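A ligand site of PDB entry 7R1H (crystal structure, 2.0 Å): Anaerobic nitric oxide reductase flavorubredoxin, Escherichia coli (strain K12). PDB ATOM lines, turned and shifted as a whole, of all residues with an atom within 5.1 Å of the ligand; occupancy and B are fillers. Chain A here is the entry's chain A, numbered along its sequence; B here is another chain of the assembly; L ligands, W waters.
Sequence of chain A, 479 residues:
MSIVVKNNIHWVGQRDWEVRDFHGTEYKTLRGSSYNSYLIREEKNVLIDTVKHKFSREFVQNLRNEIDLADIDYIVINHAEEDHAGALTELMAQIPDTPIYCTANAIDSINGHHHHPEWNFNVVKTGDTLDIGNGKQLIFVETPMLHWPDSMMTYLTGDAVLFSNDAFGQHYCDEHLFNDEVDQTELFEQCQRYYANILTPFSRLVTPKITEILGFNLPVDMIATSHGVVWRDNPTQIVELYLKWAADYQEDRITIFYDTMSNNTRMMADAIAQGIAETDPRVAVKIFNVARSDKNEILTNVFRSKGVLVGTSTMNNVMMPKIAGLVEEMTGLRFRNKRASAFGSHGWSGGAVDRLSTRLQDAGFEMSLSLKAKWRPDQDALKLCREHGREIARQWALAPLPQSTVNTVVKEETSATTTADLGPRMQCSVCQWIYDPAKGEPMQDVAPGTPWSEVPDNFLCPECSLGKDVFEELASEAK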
ATOM      1  N   ASP A 259       4.697  -3.119   0.582  1.00  0.00           N
ATOM      2  CA  ASP A 259       5.191  -4.124   1.510  1.00  0.00           C
ATOM      3  C   ASP A 259       5.792  -5.235   0.671  1.00  0.00           C
ATOM      4  O   ASP A 259       5.513  -5.344  -0.524  1.00  0.00           O
ATOM      5  CB  ASP A 259       4.103  -4.654   2.442  1.00  0.00           C
ATOM      6  CG  ASP A 259       4.664  -5.174   3.771  1.00  0.00           C
ATOM      7  OD1 ASP A 259       5.853  -5.546   3.801  1.00  0.00           O
ATOM      8  OD2 ASP A 259       3.933  -5.189   4.775  1.00  0.00           O
ATOM      9  N   THR A 260       6.652  -6.035   1.282  1.00  0.00           N
ATOM     10  CA  THR A 260       7.354  -7.064   0.544  1.00  0.00           C
ATOM     11  C   THR A 260       7.688  -8.243   1.465  1.00  0.00           C
ATOM     12  O   THR A 260       7.982  -8.050   2.633  1.00  0.00           O
ATOM     13  CB  THR A 260       8.657  -6.500  -0.075  1.00  0.00           C
ATOM     14  OG1 THR A 260       9.236  -7.472  -0.952  1.00  0.00           O
ATOM     15  CG2 THR A 260       9.668  -6.108   1.001  1.00  0.00           C
ATOM     16  N   MET A 261       7.613  -9.453   0.917  1.00  0.00           N
ATOM     17  CA  MET A 261       7.884 -10.658   1.699  1.00  0.00           C
ATOM     18  C   MET A 261       9.307 -11.169   1.471  1.00  0.00           C
ATOM     19  O   MET A 261       9.899 -11.794   2.342  1.00  0.00           O
ATOM     20  CB  MET A 261       6.881 -11.757   1.361  1.00  0.00           C
ATOM     21  CG  MET A 261       5.446 -11.497   1.834  1.00  0.00           C
ATOM     22  SD  MET A 261       4.346 -12.904   1.482  1.00  0.00           S
ATOM     23  CE  MET A 261       4.444 -12.961  -0.311  1.00  0.00           C
ATOM     24  N   SER A 262       9.841 -10.916   0.279  1.00  0.00           N
ATOM     25  CA  SER A 262      11.183 -11.365  -0.064  1.00  0.00           C
ATOM     26  C   SER A 262      11.929 -10.341  -0.937  1.00  0.00           C
ATOM     27  O   SER A 262      12.876 -10.687  -1.635  1.00  0.00           O
ATOM     28  CB  SER A 262      11.129 -12.729  -0.766  1.00  0.00           C
ATOM     29  OG  SER A 262      10.182 -12.728  -1.832  1.00  0.00           O
ATOM     30  N   ASN A 263      11.460  -9.097  -0.884  1.00  0.00           N
ATOM     31  CA  ASN A 263      12.170  -7.945  -1.447  1.00  0.00           C
ATOM     32  C   ASN A 263      12.066  -7.736  -2.960  1.00  0.00           C
ATOM     33  O   ASN A 263      12.630  -6.789  -3.497  1.00  0.00           O
ATOM     34  CB  ASN A 263      13.651  -8.020  -1.062  1.00  0.00           C
ATOM     35  CG  ASN A 263      13.869  -7.848   0.436  1.00  0.00           C
ATOM     36  OD1 ASN A 263      13.312  -6.936   1.056  1.00  0.00           O
ATOM     37  ND2 ASN A 263      14.673  -8.726   1.014  1.00  0.00           N
ATOM     38  N   ASN A 264      11.337  -8.604  -3.652  1.00  0.00           N
ATOM     39  CA  ASN A 264      11.190  -8.454  -5.093  1.00  0.00           C
ATOM     40  C   ASN A 264      10.457  -7.156  -5.461  1.00  0.00           C
ATOM     41  O   ASN A 264      10.874  -6.442  -6.375  1.00  0.00           O
ATOM     42  CB  ASN A 264      10.460  -9.658  -5.677  1.00  0.00           C
ATOM     43  CG  ASN A 264      11.243 -10.943  -5.503  1.00  0.00           C
ATOM     44  OD1 ASN A 264      12.471 -10.916  -5.390  1.00  0.00           O
ATOM     45  ND2 ASN A 264      10.548 -12.078  -5.458  1.00  0.00           N
ATOM     46  N   THR A 265       9.396  -6.848  -4.735  1.00  0.00           N
ATOM     47  CA  THR A 265       8.639  -5.618  -4.976  1.00  0.00           C
ATOM     48  C   THR A 265       9.461  -4.395  -4.588  1.00  0.00           C
ATOM     49  O   THR A 265       9.315  -3.328  -5.190  1.00  0.00           O
ATOM     50  CB  THR A 265       7.306  -5.634  -4.203  1.00  0.00           C
ATOM     51  OG1 THR A 265       6.480  -6.683  -4.700  1.00  0.00           O
ATOM     52  CG2 THR A 265       6.560  -4.304  -4.364  1.00  0.00           C
ATOM     53  N   ARG A 266      10.347  -4.554  -3.614  1.00  0.00           N
ATOM     54  CA  ARG A 266      11.249  -3.481  -3.234  1.00  0.00           C
ATOM     55  C   ARG A 266      12.185  -3.129  -4.394  1.00  0.00           C
ATOM     56  O   ARG A 266      12.406  -1.955  -4.698  1.00  0.00           O
ATOM     57  CB  ARG A 266      12.081  -3.847  -2.005  1.00  0.00           C
ATOM     58  CG  ARG A 266      13.148  -2.808  -1.700  1.00  0.00           C
ATOM     59  CD  ARG A 266      14.090  -3.236  -0.585  1.00  0.00           C
ATOM     60  NE  ARG A 266      15.089  -2.195  -0.340  1.00  0.00           N
ATOM     61  CZ  ARG A 266      15.917  -2.182   0.691  1.00  0.00           C
ATOM     62  NH1 ARG A 266      15.867  -3.146   1.605  1.00  0.00           N
ATOM     63  NH2 ARG A 266      16.794  -1.187   0.823  1.00  0.00           N
ATOM     64  N   SER A 313       3.118  -7.714  -3.291  1.00  0.00           N
ATOM     65  CA  SER A 313       3.203  -9.019  -3.915  1.00  0.00           C
ATOM     66  C   SER A 313       1.887  -9.747  -3.667  1.00  0.00           C
ATOM     67  O   SER A 313       1.056  -9.284  -2.889  1.00  0.00           O
ATOM     68  CB  SER A 313       4.388  -9.820  -3.368  1.00  0.00           C
ATOM     69  OG  SER A 313       4.364  -9.893  -1.958  1.00  0.00           O
ATOM     70  N   THR A 314       1.700 -10.878  -4.327  1.00  0.00           N
ATOM     71  CA  THR A 314       0.508 -11.677  -4.116  1.00  0.00           C
ATOM     72  C   THR A 314       0.732 -12.666  -2.993  1.00  0.00           C
ATOM     73  O   THR A 314       1.673 -13.467  -3.033  1.00  0.00           O
ATOM     74  CB  THR A 314       0.069 -12.425  -5.377  1.00  0.00           C
ATOM     75  OG1 THR A 314      -0.265 -11.475  -6.401  1.00  0.00           O
ATOM     76  CG2 THR A 314      -1.144 -13.290  -5.074  1.00  0.00           C
ATOM     77  N   MET A 315      -0.133 -12.599  -1.987  1.00  0.00           N
ATOM     78  CA  MET A 315      -0.048 -13.449  -0.817  1.00  0.00           C
ATOM     79  C   MET A 315      -1.376 -14.166  -0.617  1.00  0.00           C
ATOM     80  O   MET A 315      -2.373 -13.556  -0.216  1.00  0.00           O
ATOM     81  CB  MET A 315       0.309 -12.601   0.415  1.00  0.00           C
ATOM     82  CG  MET A 315       0.247 -13.314   1.746  1.00  0.00           C
ATOM     83  SD  MET A 315       0.558 -12.153   3.093  1.00  0.00           S
ATOM     84  CE  MET A 315       0.375 -13.211   4.532  1.00  0.00           C
ATOM     85  N   ASN A 316      -1.393 -15.465  -0.902  1.00  0.00           N
ATOM     86  CA  ASN A 316      -2.608 -16.264  -0.817  1.00  0.00           C
ATOM     87  C   ASN A 316      -3.717 -15.666  -1.677  1.00  0.00           C
ATOM     88  O   ASN A 316      -4.858 -15.513  -1.218  1.00  0.00           O
ATOM     89  CB  ASN A 316      -3.080 -16.384   0.636  1.00  0.00           C
ATOM     90  CG  ASN A 316      -2.047 -17.035   1.528  1.00  0.00           C
ATOM     91  OD1 ASN A 316      -1.333 -17.950   1.125  1.00  0.00           O
ATOM     92  ND2 ASN A 316      -1.974 -16.573   2.772  1.00  0.00           N
ATOM     93  N   ASN A 317      -3.374 -15.308  -2.912  1.00  0.00           N
ATOM     94  CA  ASN A 317      -4.324 -14.764  -3.882  1.00  0.00           C
ATOM     95  C   ASN A 317      -4.831 -13.351  -3.569  1.00  0.00           C
ATOM     96  O   ASN A 317      -5.607 -12.787  -4.331  1.00  0.00           O
ATOM     97  CB  ASN A 317      -5.532 -15.707  -4.027  1.00  0.00           C
ATOM     98  CG  ASN A 317      -5.144 -17.081  -4.545  1.00  0.00           C
ATOM     99  OD1 ASN A 317      -4.671 -17.212  -5.677  1.00  0.00           O
ATOM    100  ND2 ASN A 317      -5.334 -18.103  -3.722  1.00  0.00           N
ATOM    101  N   MET A 320      -0.909  -7.998   0.408  1.00  0.00           N
ATOM    102  CA  MET A 320      -0.372  -8.016   1.755  1.00  0.00           C
ATOM    103  C   MET A 320      -1.208  -7.092   2.641  1.00  0.00           C
ATOM    104  O   MET A 320      -1.618  -6.018   2.198  1.00  0.00           O
ATOM    105  CB  MET A 320       1.093  -7.617   1.746  1.00  0.00           C
ATOM    106  CG  MET A 320       1.949  -8.560   0.915  1.00  0.00           C
ATOM    107  SD  MET A 320       3.714  -8.232   1.048  1.00  0.00           S
ATOM    108  CE  MET A 320       3.951  -8.469   2.808  1.00  0.00           C
ATOM    109  N   SER A 345       5.312  -7.965  -7.349  1.00  0.00           N
ATOM    110  CA  SER A 345       5.752  -9.251  -7.861  1.00  0.00           C
ATOM    111  C   SER A 345       4.773 -10.376  -7.528  1.00  0.00           C
ATOM    112  O   SER A 345       3.925 -10.232  -6.642  1.00  0.00           O
ATOM    113  CB  SER A 345       7.145  -9.576  -7.312  1.00  0.00           C
ATOM    114  OG  SER A 345       7.600 -10.842  -7.754  1.00  0.00           O
ATOM    115  N   HIS A 346       4.897 -11.491  -8.222  1.00  0.00           N
ATOM    116  CA  HIS A 346       4.047 -12.645  -7.955  1.00  0.00           C
ATOM    117  C   HIS A 346       4.808 -13.930  -8.254  1.00  0.00           C
ATOM    118  O   HIS A 346       5.835 -13.901  -8.943  1.00  0.00           O
ATOM    119  CB  HIS A 346       2.756 -12.591  -8.778  1.00  0.00           C
ATOM    120  CG  HIS A 346       2.983 -12.800 -10.242  1.00  0.00           C
ATOM    121  ND1 HIS A 346       3.270 -11.772 -11.113  1.00  0.00           N
ATOM    122  CD2 HIS A 346       2.971 -13.934 -10.992  1.00  0.00           C
ATOM    123  CE1 HIS A 346       3.419 -12.263 -12.330  1.00  0.00           C
ATOM    124  NE2 HIS A 346       3.245 -13.574 -12.286  1.00  0.00           N
ATOM    125  N   GLY A 347       4.290 -15.052  -7.759  1.00  0.00           N
ATOM    126  CA  GLY A 347       4.923 -16.349  -7.944  1.00  0.00           C
ATOM    127  C   GLY A 347       4.344 -17.202  -9.064  1.00  0.00           C
ATOM    128  O   GLY A 347       5.080 -17.831  -9.817  1.00  0.00           O
ATOM    129  N   TRP A 348       3.021 -17.253  -9.156  1.00  0.00           N
ATOM    130  CA  TRP A 348       2.394 -18.045 -10.215  1.00  0.00           C
ATOM    131  C   TRP A 348       1.190 -17.336 -10.833  1.00  0.00           C
ATOM    132  O   TRP A 348       1.319 -16.721 -11.893  1.00  0.00           O
ATOM    133  CB  TRP A 348       1.996 -19.433  -9.697  1.00  0.00           C
ATOM    134  CG  TRP A 348       1.393 -19.479  -8.320  1.00  0.00           C
ATOM    135  CD1 TRP A 348       0.072 -19.612  -7.996  1.00  0.00           C
ATOM    136  CD2 TRP A 348       2.099 -19.420  -7.067  1.00  0.00           C
ATOM    137  NE1 TRP A 348      -0.092 -19.634  -6.632  1.00  0.00           N
ATOM    138  CE2 TRP A 348       1.137 -19.510  -6.036  1.00  0.00           C
ATOM    139  CE3 TRP A 348       3.449 -19.301  -6.713  1.00  0.00           C
ATOM    140  CZ2 TRP A 348       1.482 -19.486  -4.690  1.00  0.00           C
ATOM    141  CZ3 TRP A 348       3.785 -19.268  -5.373  1.00  0.00           C
ATOM    142  CH2 TRP A 348       2.800 -19.360  -4.376  1.00  0.00           C
ATOM    143  N   SER A 349       0.022 -17.415 -10.206  1.00  0.00           N
ATOM    144  CA  SER A 349      -1.200 -16.861 -10.798  1.00  0.00           C
ATOM    145  C   SER A 349      -1.409 -15.374 -10.467  1.00  0.00           C
ATOM    146  O   SER A 349      -2.130 -14.682 -11.187  1.00  0.00           O
ATOM    147  CB  SER A 349      -2.420 -17.670 -10.358  1.00  0.00           C
ATOM    148  OG  SER A 349      -2.457 -17.846  -8.949  1.00  0.00           O
ATOM    149  N   GLY A 350      -0.785 -14.896  -9.407  1.00  0.00           N
ATOM    150  CA  GLY A 350      -0.871 -13.494  -9.035  1.00  0.00           C
ATOM    151  C   GLY A 350      -2.294 -13.014  -8.758  1.00  0.00           C
ATOM    152  O   GLY A 350      -3.146 -13.789  -8.313  1.00  0.00           O
ATOM    153  N   LYS A 374       7.495 -11.266 -12.347  1.00  0.00           N
ATOM    154  CA  LYS A 374       7.457 -12.592 -11.760  1.00  0.00           C
ATOM    155  C   LYS A 374       8.737 -12.880 -10.983  1.00  0.00           C
ATOM    156  O   LYS A 374       9.837 -12.683 -11.489  1.00  0.00           O
ATOM    157  CB  LYS A 374       7.269 -13.651 -12.851  1.00  0.00           C
ATOM    158  CG  LYS A 374       6.905 -15.034 -12.343  1.00  0.00           C
ATOM    159  CD  LYS A 374       6.835 -16.044 -13.483  1.00  0.00           C
ATOM    160  CE  LYS A 374       6.376 -17.410 -12.976  1.00  0.00           C
ATOM    161  NZ  LYS A 374       6.355 -18.435 -14.063  1.00  0.00           N
ATOM    162  N   TRP A 375       8.575 -13.343  -9.741  1.00  0.00           N
ATOM    163  CA  TRP A 375       9.708 -13.604  -8.847  1.00  0.00           C
ATOM    164  C   TRP A 375      10.641 -12.387  -8.765  1.00  0.00           C
ATOM    165  O   TRP A 375      10.190 -11.240  -8.779  1.00  0.00           O
ATOM    166  CB  TRP A 375      10.493 -14.831  -9.317  1.00  0.00           C
ATOM    167  CG  TRP A 375       9.675 -16.102  -9.401  1.00  0.00           C
ATOM    168  CD1 TRP A 375       9.456 -16.872 -10.514  1.00  0.00           C
ATOM    169  CD2 TRP A 375       8.956 -16.753  -8.339  1.00  0.00           C
ATOM    170  NE1 TRP A 375       8.670 -17.957 -10.206  1.00  0.00           N
ATOM    171  CE2 TRP A 375       8.342 -17.901  -8.880  1.00  0.00           C
ATOM    172  CE3 TRP A 375       8.776 -16.464  -6.969  1.00  0.00           C
ATOM    173  CZ2 TRP A 375       7.567 -18.765  -8.102  1.00  0.00           C
ATOM    174  CZ3 TRP A 375       8.006 -17.327  -6.212  1.00  0.00           C
ATOM    175  CH2 TRP A 375       7.410 -18.461  -6.775  1.00  0.00           C
ATOM    176  N   ARG A 376      11.945 -12.641  -8.683  1.00  0.00           N
ATOM    177  CA  ARG A 376      12.928 -11.568  -8.607  1.00  0.00           C
ATOM    178  C   ARG A 376      13.249 -11.027  -9.992  1.00  0.00           C
ATOM    179  O   ARG A 376      13.587 -11.791 -10.900  1.00  0.00           O
ATOM    180  CB  ARG A 376      14.210 -12.045  -7.911  1.00  0.00           C
ATOM    181  CG  ARG A 376      15.246 -10.946  -7.731  1.00  0.00           C
ATOM    182  CD  ARG A 376      16.404 -11.377  -6.843  1.00  0.00           C
ATOM    183  NE  ARG A 376      17.272 -12.363  -7.469  1.00  0.00           N
ATOM    184  CZ  ARG A 376      18.240 -12.055  -8.327  1.00  0.00           C
ATOM    185  NH1 ARG A 376      18.467 -10.789  -8.666  1.00  0.00           N
ATOM    186  NH2 ARG A 376      18.982 -13.023  -8.860  1.00  0.00           N
ATOM    187  N   HIS B  23       8.852 -13.666   5.919  1.00  0.00           N
ATOM    188  CA  HIS B  23       7.955 -13.113   4.917  1.00  0.00           C
ATOM    189  C   HIS B  23       7.654 -11.649   5.204  1.00  0.00           C
ATOM    190  O   HIS B  23       6.497 -11.259   5.392  1.00  0.00           O
ATOM    191  CB  HIS B  23       6.654 -13.921   4.858  1.00  0.00           C
ATOM    192  CG  HIS B  23       6.852 -15.357   4.472  1.00  0.00           C
ATOM    193  ND1 HIS B  23       5.962 -16.348   4.823  1.00  0.00           N
ATOM    194  CD2 HIS B  23       7.830 -15.961   3.760  1.00  0.00           C
ATOM    195  CE1 HIS B  23       6.385 -17.506   4.357  1.00  0.00           C
ATOM    196  NE2 HIS B  23       7.518 -17.300   3.706  1.00  0.00           N
ATOM    197  N   GLU B  81      12.017 -21.675  -2.007  1.00  0.00           N
ATOM    198  CA  GLU B  81      11.865 -20.444  -1.252  1.00  0.00           C
ATOM    199  C   GLU B  81      13.236 -20.085  -0.682  1.00  0.00           C
ATOM    200  O   GLU B  81      14.038 -20.966  -0.388  1.00  0.00           O
ATOM    201  CB  GLU B  81      10.815 -20.579  -0.145  1.00  0.00           C
ATOM    202  CG  GLU B  81      10.416 -19.239   0.465  1.00  0.00           C
ATOM    203  CD  GLU B  81       9.056 -19.266   1.119  1.00  0.00           C
ATOM    204  OE1 GLU B  81       8.502 -20.356   1.348  1.00  0.00           O
ATOM    205  OE2 GLU B  81       8.531 -18.169   1.421  1.00  0.00           O
ATOM    206  N   HIS B 113      14.518 -16.765  -8.903  1.00  0.00           N
ATOM    207  CA  HIS B 113      15.281 -16.116  -7.842  1.00  0.00           C
ATOM    208  C   HIS B 113      16.762 -15.958  -8.183  1.00  0.00           C
ATOM    209  O   HIS B 113      17.393 -14.954  -7.836  1.00  0.00           O
ATOM    210  CB  HIS B 113      15.142 -16.901  -6.536  1.00  0.00           C
ATOM    211  CG  HIS B 113      13.745 -16.910  -5.993  1.00  0.00           C
ATOM    212  ND1 HIS B 113      12.769 -17.769  -6.470  1.00  0.00           N
ATOM    213  CD2 HIS B 113      13.157 -16.174  -5.027  1.00  0.00           C
ATOM    214  CE1 HIS B 113      11.647 -17.559  -5.813  1.00  0.00           C
ATOM    215  NE2 HIS B 113      11.852 -16.602  -4.923  1.00  0.00           N
ATOM    216  N   HIS B 147       3.745 -25.863   0.292  1.00  0.00           N
ATOM    217  CA  HIS B 147       2.744 -24.821   0.064  1.00  0.00           C
ATOM    218  C   HIS B 147       2.975 -24.014  -1.212  1.00  0.00           C
ATOM    219  O   HIS B 147       2.228 -23.065  -1.487  1.00  0.00           O
ATOM    220  CB  HIS B 147       2.707 -23.879   1.274  1.00  0.00           C
ATOM    221  CG  HIS B 147       3.997 -23.160   1.523  1.00  0.00           C
ATOM    222  ND1 HIS B 147       4.208 -21.864   1.122  1.00  0.00           N
ATOM    223  CD2 HIS B 147       5.147 -23.563   2.115  1.00  0.00           C
ATOM    224  CE1 HIS B 147       5.434 -21.490   1.461  1.00  0.00           C
ATOM    225  NE2 HIS B 147       6.016 -22.502   2.064  1.00  0.00           N
ATOM    226  N   TRP B 148       3.990 -24.368  -1.985  1.00  0.00           N
ATOM    227  CA  TRP B 148       4.256 -23.707  -3.266  1.00  0.00           C
ATOM    228  C   TRP B 148       4.040 -24.657  -4.432  1.00  0.00           C
ATOM    229  O   TRP B 148       3.967 -25.866  -4.244  1.00  0.00           O
ATOM    230  CB  TRP B 148       5.691 -23.169  -3.320  1.00  0.00           C
ATOM    231  CG  TRP B 148       5.856 -21.764  -2.809  1.00  0.00           C
ATOM    232  CD1 TRP B 148       4.973 -21.056  -2.052  1.00  0.00           C
ATOM    233  CD2 TRP B 148       6.985 -20.914  -3.001  1.00  0.00           C
ATOM    234  NE1 TRP B 148       5.478 -19.806  -1.764  1.00  0.00           N
ATOM    235  CE2 TRP B 148       6.722 -19.697  -2.345  1.00  0.00           C
ATOM    236  CE3 TRP B 148       8.211 -21.058  -3.678  1.00  0.00           C
ATOM    237  CZ2 TRP B 148       7.617 -18.635  -2.334  1.00  0.00           C
ATOM    238  CZ3 TRP B 148       9.099 -19.997  -3.673  1.00  0.00           C
ATOM    239  CH2 TRP B 148       8.802 -18.795  -3.009  1.00  0.00           C
HETATM  240  N1  LIG L   1       2.286 -16.029  -5.798  1.00  0.00           N
HETATM  241  C1  LIG L   1       1.140 -16.056  -6.561  1.00  0.00           C
HETATM  242  O1  LIG L   1       1.216 -15.870  -7.775  1.00  0.00           O
HETATM  243  N2  LIG L   1      -0.087 -16.274  -5.969  1.00  0.00           N
HETATM  244  C2  LIG L   1      -0.174 -16.477  -4.606  1.00  0.00           C
HETATM  245  O2  LIG L   1      -1.263 -16.683  -4.079  1.00  0.00           O
HETATM  246  C3  LIG L   1       0.989 -16.458  -3.830  1.00  0.00           C
HETATM  247  N3  LIG L   1       0.917 -16.658  -2.469  1.00  0.00           N
HETATM  248  C4  LIG L   1       2.078 -16.639  -1.707  1.00  0.00           C
HETATM  249  C5  LIG L   1       2.007 -16.839  -0.331  1.00  0.00           C
HETATM  250  C6  LIG L   1       3.173 -16.809   0.423  1.00  0.00           C
HETATM  251  C7  LIG L   1       3.112 -17.032   1.911  1.00  0.00           C
HETATM  252  C8  LIG L   1       4.398 -16.581  -0.183  1.00  0.00           C
HETATM  253  C9  LIG L   1       5.656 -16.560   0.636  1.00  0.00           C
HETATM  254  C10 LIG L   1       4.470 -16.381  -1.559  1.00  0.00           C
HETATM  255  C11 LIG L   1       3.302 -16.411  -2.327  1.00  0.00           C
HETATM  256  N4  LIG L   1       3.367 -16.202  -3.681  1.00  0.00           N
HETATM  257  C12 LIG L   1       2.214 -16.230  -4.437  1.00  0.00           C
HETATM  258  C13 LIG L   1       4.692 -15.957  -4.358  1.00  0.00           C
HETATM  259  C14 LIG L   1       5.161 -14.517  -4.177  1.00  0.00           C
HETATM  260  O3  LIG L   1       4.180 -13.617  -4.665  1.00  0.00           O
HETATM  261  C15 LIG L   1       6.483 -14.312  -4.904  1.00  0.00           C
HETATM  262  O4  LIG L   1       7.523 -14.917  -4.145  1.00  0.00           O
HETATM  263  C16 LIG L   1       6.807 -12.832  -5.124  1.00  0.00           C
HETATM  264  O5  LIG L   1       7.789 -12.730  -6.135  1.00  0.00           O
HETATM  265  C17 LIG L   1       7.340 -12.182  -3.850  1.00  0.00           C
HETATM  266  O6  LIG L   1       7.281 -10.772  -3.934  1.00  0.00           O
HETATM  267  P1  LIG L   1       7.927  -9.901  -2.740  1.00  0.00           P
HETATM  268  O7  LIG L   1       7.978  -8.437  -3.121  1.00  0.00           O
HETATM  269  O8  LIG L   1       7.108 -10.087  -1.493  1.00  0.00           O
HETATM  270  O9  LIG L   1       9.350 -10.365  -2.507  1.00  0.00           O
HETATM  271  O   HOH W   1       9.959 -14.774  -4.016  1.00  0.00           O
HETATM  272  O   HOH W   2      -2.428 -19.423  -3.360  1.00  0.00           O
HETATM  273  O   HOH W   3      -0.506 -18.879  -1.064  1.00  0.00           O
HETATM  274  O   HOH W   4       7.913 -14.462  -1.356  1.00  0.00           O
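Water W1 lies within hydrogen-bond range of O4 of the ligand (2.4 Å), NE2 of His 113 of chain B (2.8 Å), OG of Ser 262 (3.0 Å) and ND2 of Asn 264 (3.1 Å). Water W4 lies within hydrogen-bond range of O4 of the ligand (2.9 Å) and OG of Ser 262 (2.9 Å). Water W3 lies within hydrogen-bond range of the side-chain amide oxygen (OD1) of Asn 316 (2.5 Å) and a nitrogen (N3) of the ligand (3.0 Å). Water W2 lies within hydrogen-bond range of O2 of the ligand (3.1 Å) and ND2 of Asn 317 (3.2 Å).
N of Thr 314 sits at hydrogen-bond distance from O of Ser 345. The side-chain hydroxyl of Ser 345 is in hydrogen-bond range of the backbone carbonyl oxygen of Trp 375, at 2.8 Å. The side-chain hydroxyl (OG1) of Thr 260 sits at hydrogen-bond distance from the backbone NH (N) of Asn 263. N of Thr 260 lies within hydrogen-bond range of SD of Met 320, at 3.7 Å. The side-chain sulfur (SD) of Met 320 sits at hydrogen-bond distance from the side-chain hydroxyl (OG) of Ser 313, 3.5 Å away. The backbone carbonyl oxygen (O) of His 346 lies within hydrogen-bond range of the backbone NH (N) of Trp 375 (2.9 Å). The side-chain carboxylate (OE2) of Glu 81 of chain B sits at hydrogen-bond distance from a ring nitrogen (NE2) of His 23 of chain B (2.6 Å). OE1 of Glu 81 of chain B sits close to NE2 of His 147 of chain B (3.4 Å).
CA of Met 315 touches N3 of the ligand (3.7 Å). CA of His 346 touches O3 of the ligand, 3.4 Å away. CZ3 of Trp 375 touches O4 of the ligand, at 3.2 Å. His 23 of chain B touches the ligand (NE2 to C9, 3.7 Å). Glu 81 of chain B touches the ligand (OE2 to C9, 3.4 Å). NE1 of Trp 148 of chain B touches C10 of the ligand, 3.6 Å away. Hydrophobic or aromatic side chains that line the ligand: Met 261, His 346, Trp 348, Trp 375, His 23 of chain B and Trp 148 of chain B. Of the 28 residues printed, 21 come within 4 Å of the ligand. The nearest printed residue that does not touch the ligand is Arg 266 (4.6 Å).
The side-chain hydroxyl of Ser 345 is in hydrogen-bond range of an oxygen (O5) of the ligand (2.5 Å). O8 of the ligand sits at hydrogen-bond distance from N of Met 261 (2.5 Å). N of Ser 262 sits at hydrogen-bond distance from O9 of the ligand (2.9 Å). An oxygen (O9) of the ligand sits at hydrogen-bond distance from the side-chain hydroxyl (OG) of Ser 262. The backbone NH of Trp 348 is in hydrogen-bond range of an oxygen (O1) of the ligand. The backbone NH of Thr 265 sits at hydrogen-bond distance from an oxygen (O7) of the ligand, 2.7 Å away. OG1 of Thr 265 lies within hydrogen-bond range of O7 of the ligand, 2.8 Å away. The side-chain hydroxyl (OG1) of Thr 260 lies within hydrogen-bond range of an oxygen (O7) of the ligand (2.7 Å). An oxygen (O1) of the ligand is in hydrogen-bond range of the backbone NH (N) of Gly 350 (2.8 Å). The backbone NH (N) of Asn 317 sits at hydrogen-bond distance from an oxygen (O2) of the ligand (2.8 Å). An oxygen (O8) of the ligand is in hydrogen-bond range of the side-chain hydroxyl (OG) of Ser 313, 2.8 Å away. The backbone NH of Asn 264 is in hydrogen-bond range of an oxygen (O9) of the ligand, 2.9 Å away. The side-chain amide nitrogen of Asn 264 lies within hydrogen-bond range of an oxygen (O5) of the ligand, at 2.9 Å. N of Asn 263 is in hydrogen-bond range of O9 of the ligand, 2.9 Å away. A nitrogen (N1) of the ligand lies within hydrogen-bond range of the backbone NH of Gly 347 (3.0 Å). O3 of the ligand sits at hydrogen-bond distance from O of Thr 314. The backbone NH (N) of Asn 316 sits at hydrogen-bond distance from a nitrogen (N3) of the ligand, 3.0 Å away. An oxygen (O1) of the ligand lies within hydrogen-bond range of the backbone NH of Ser 349, at 3.1 Å.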
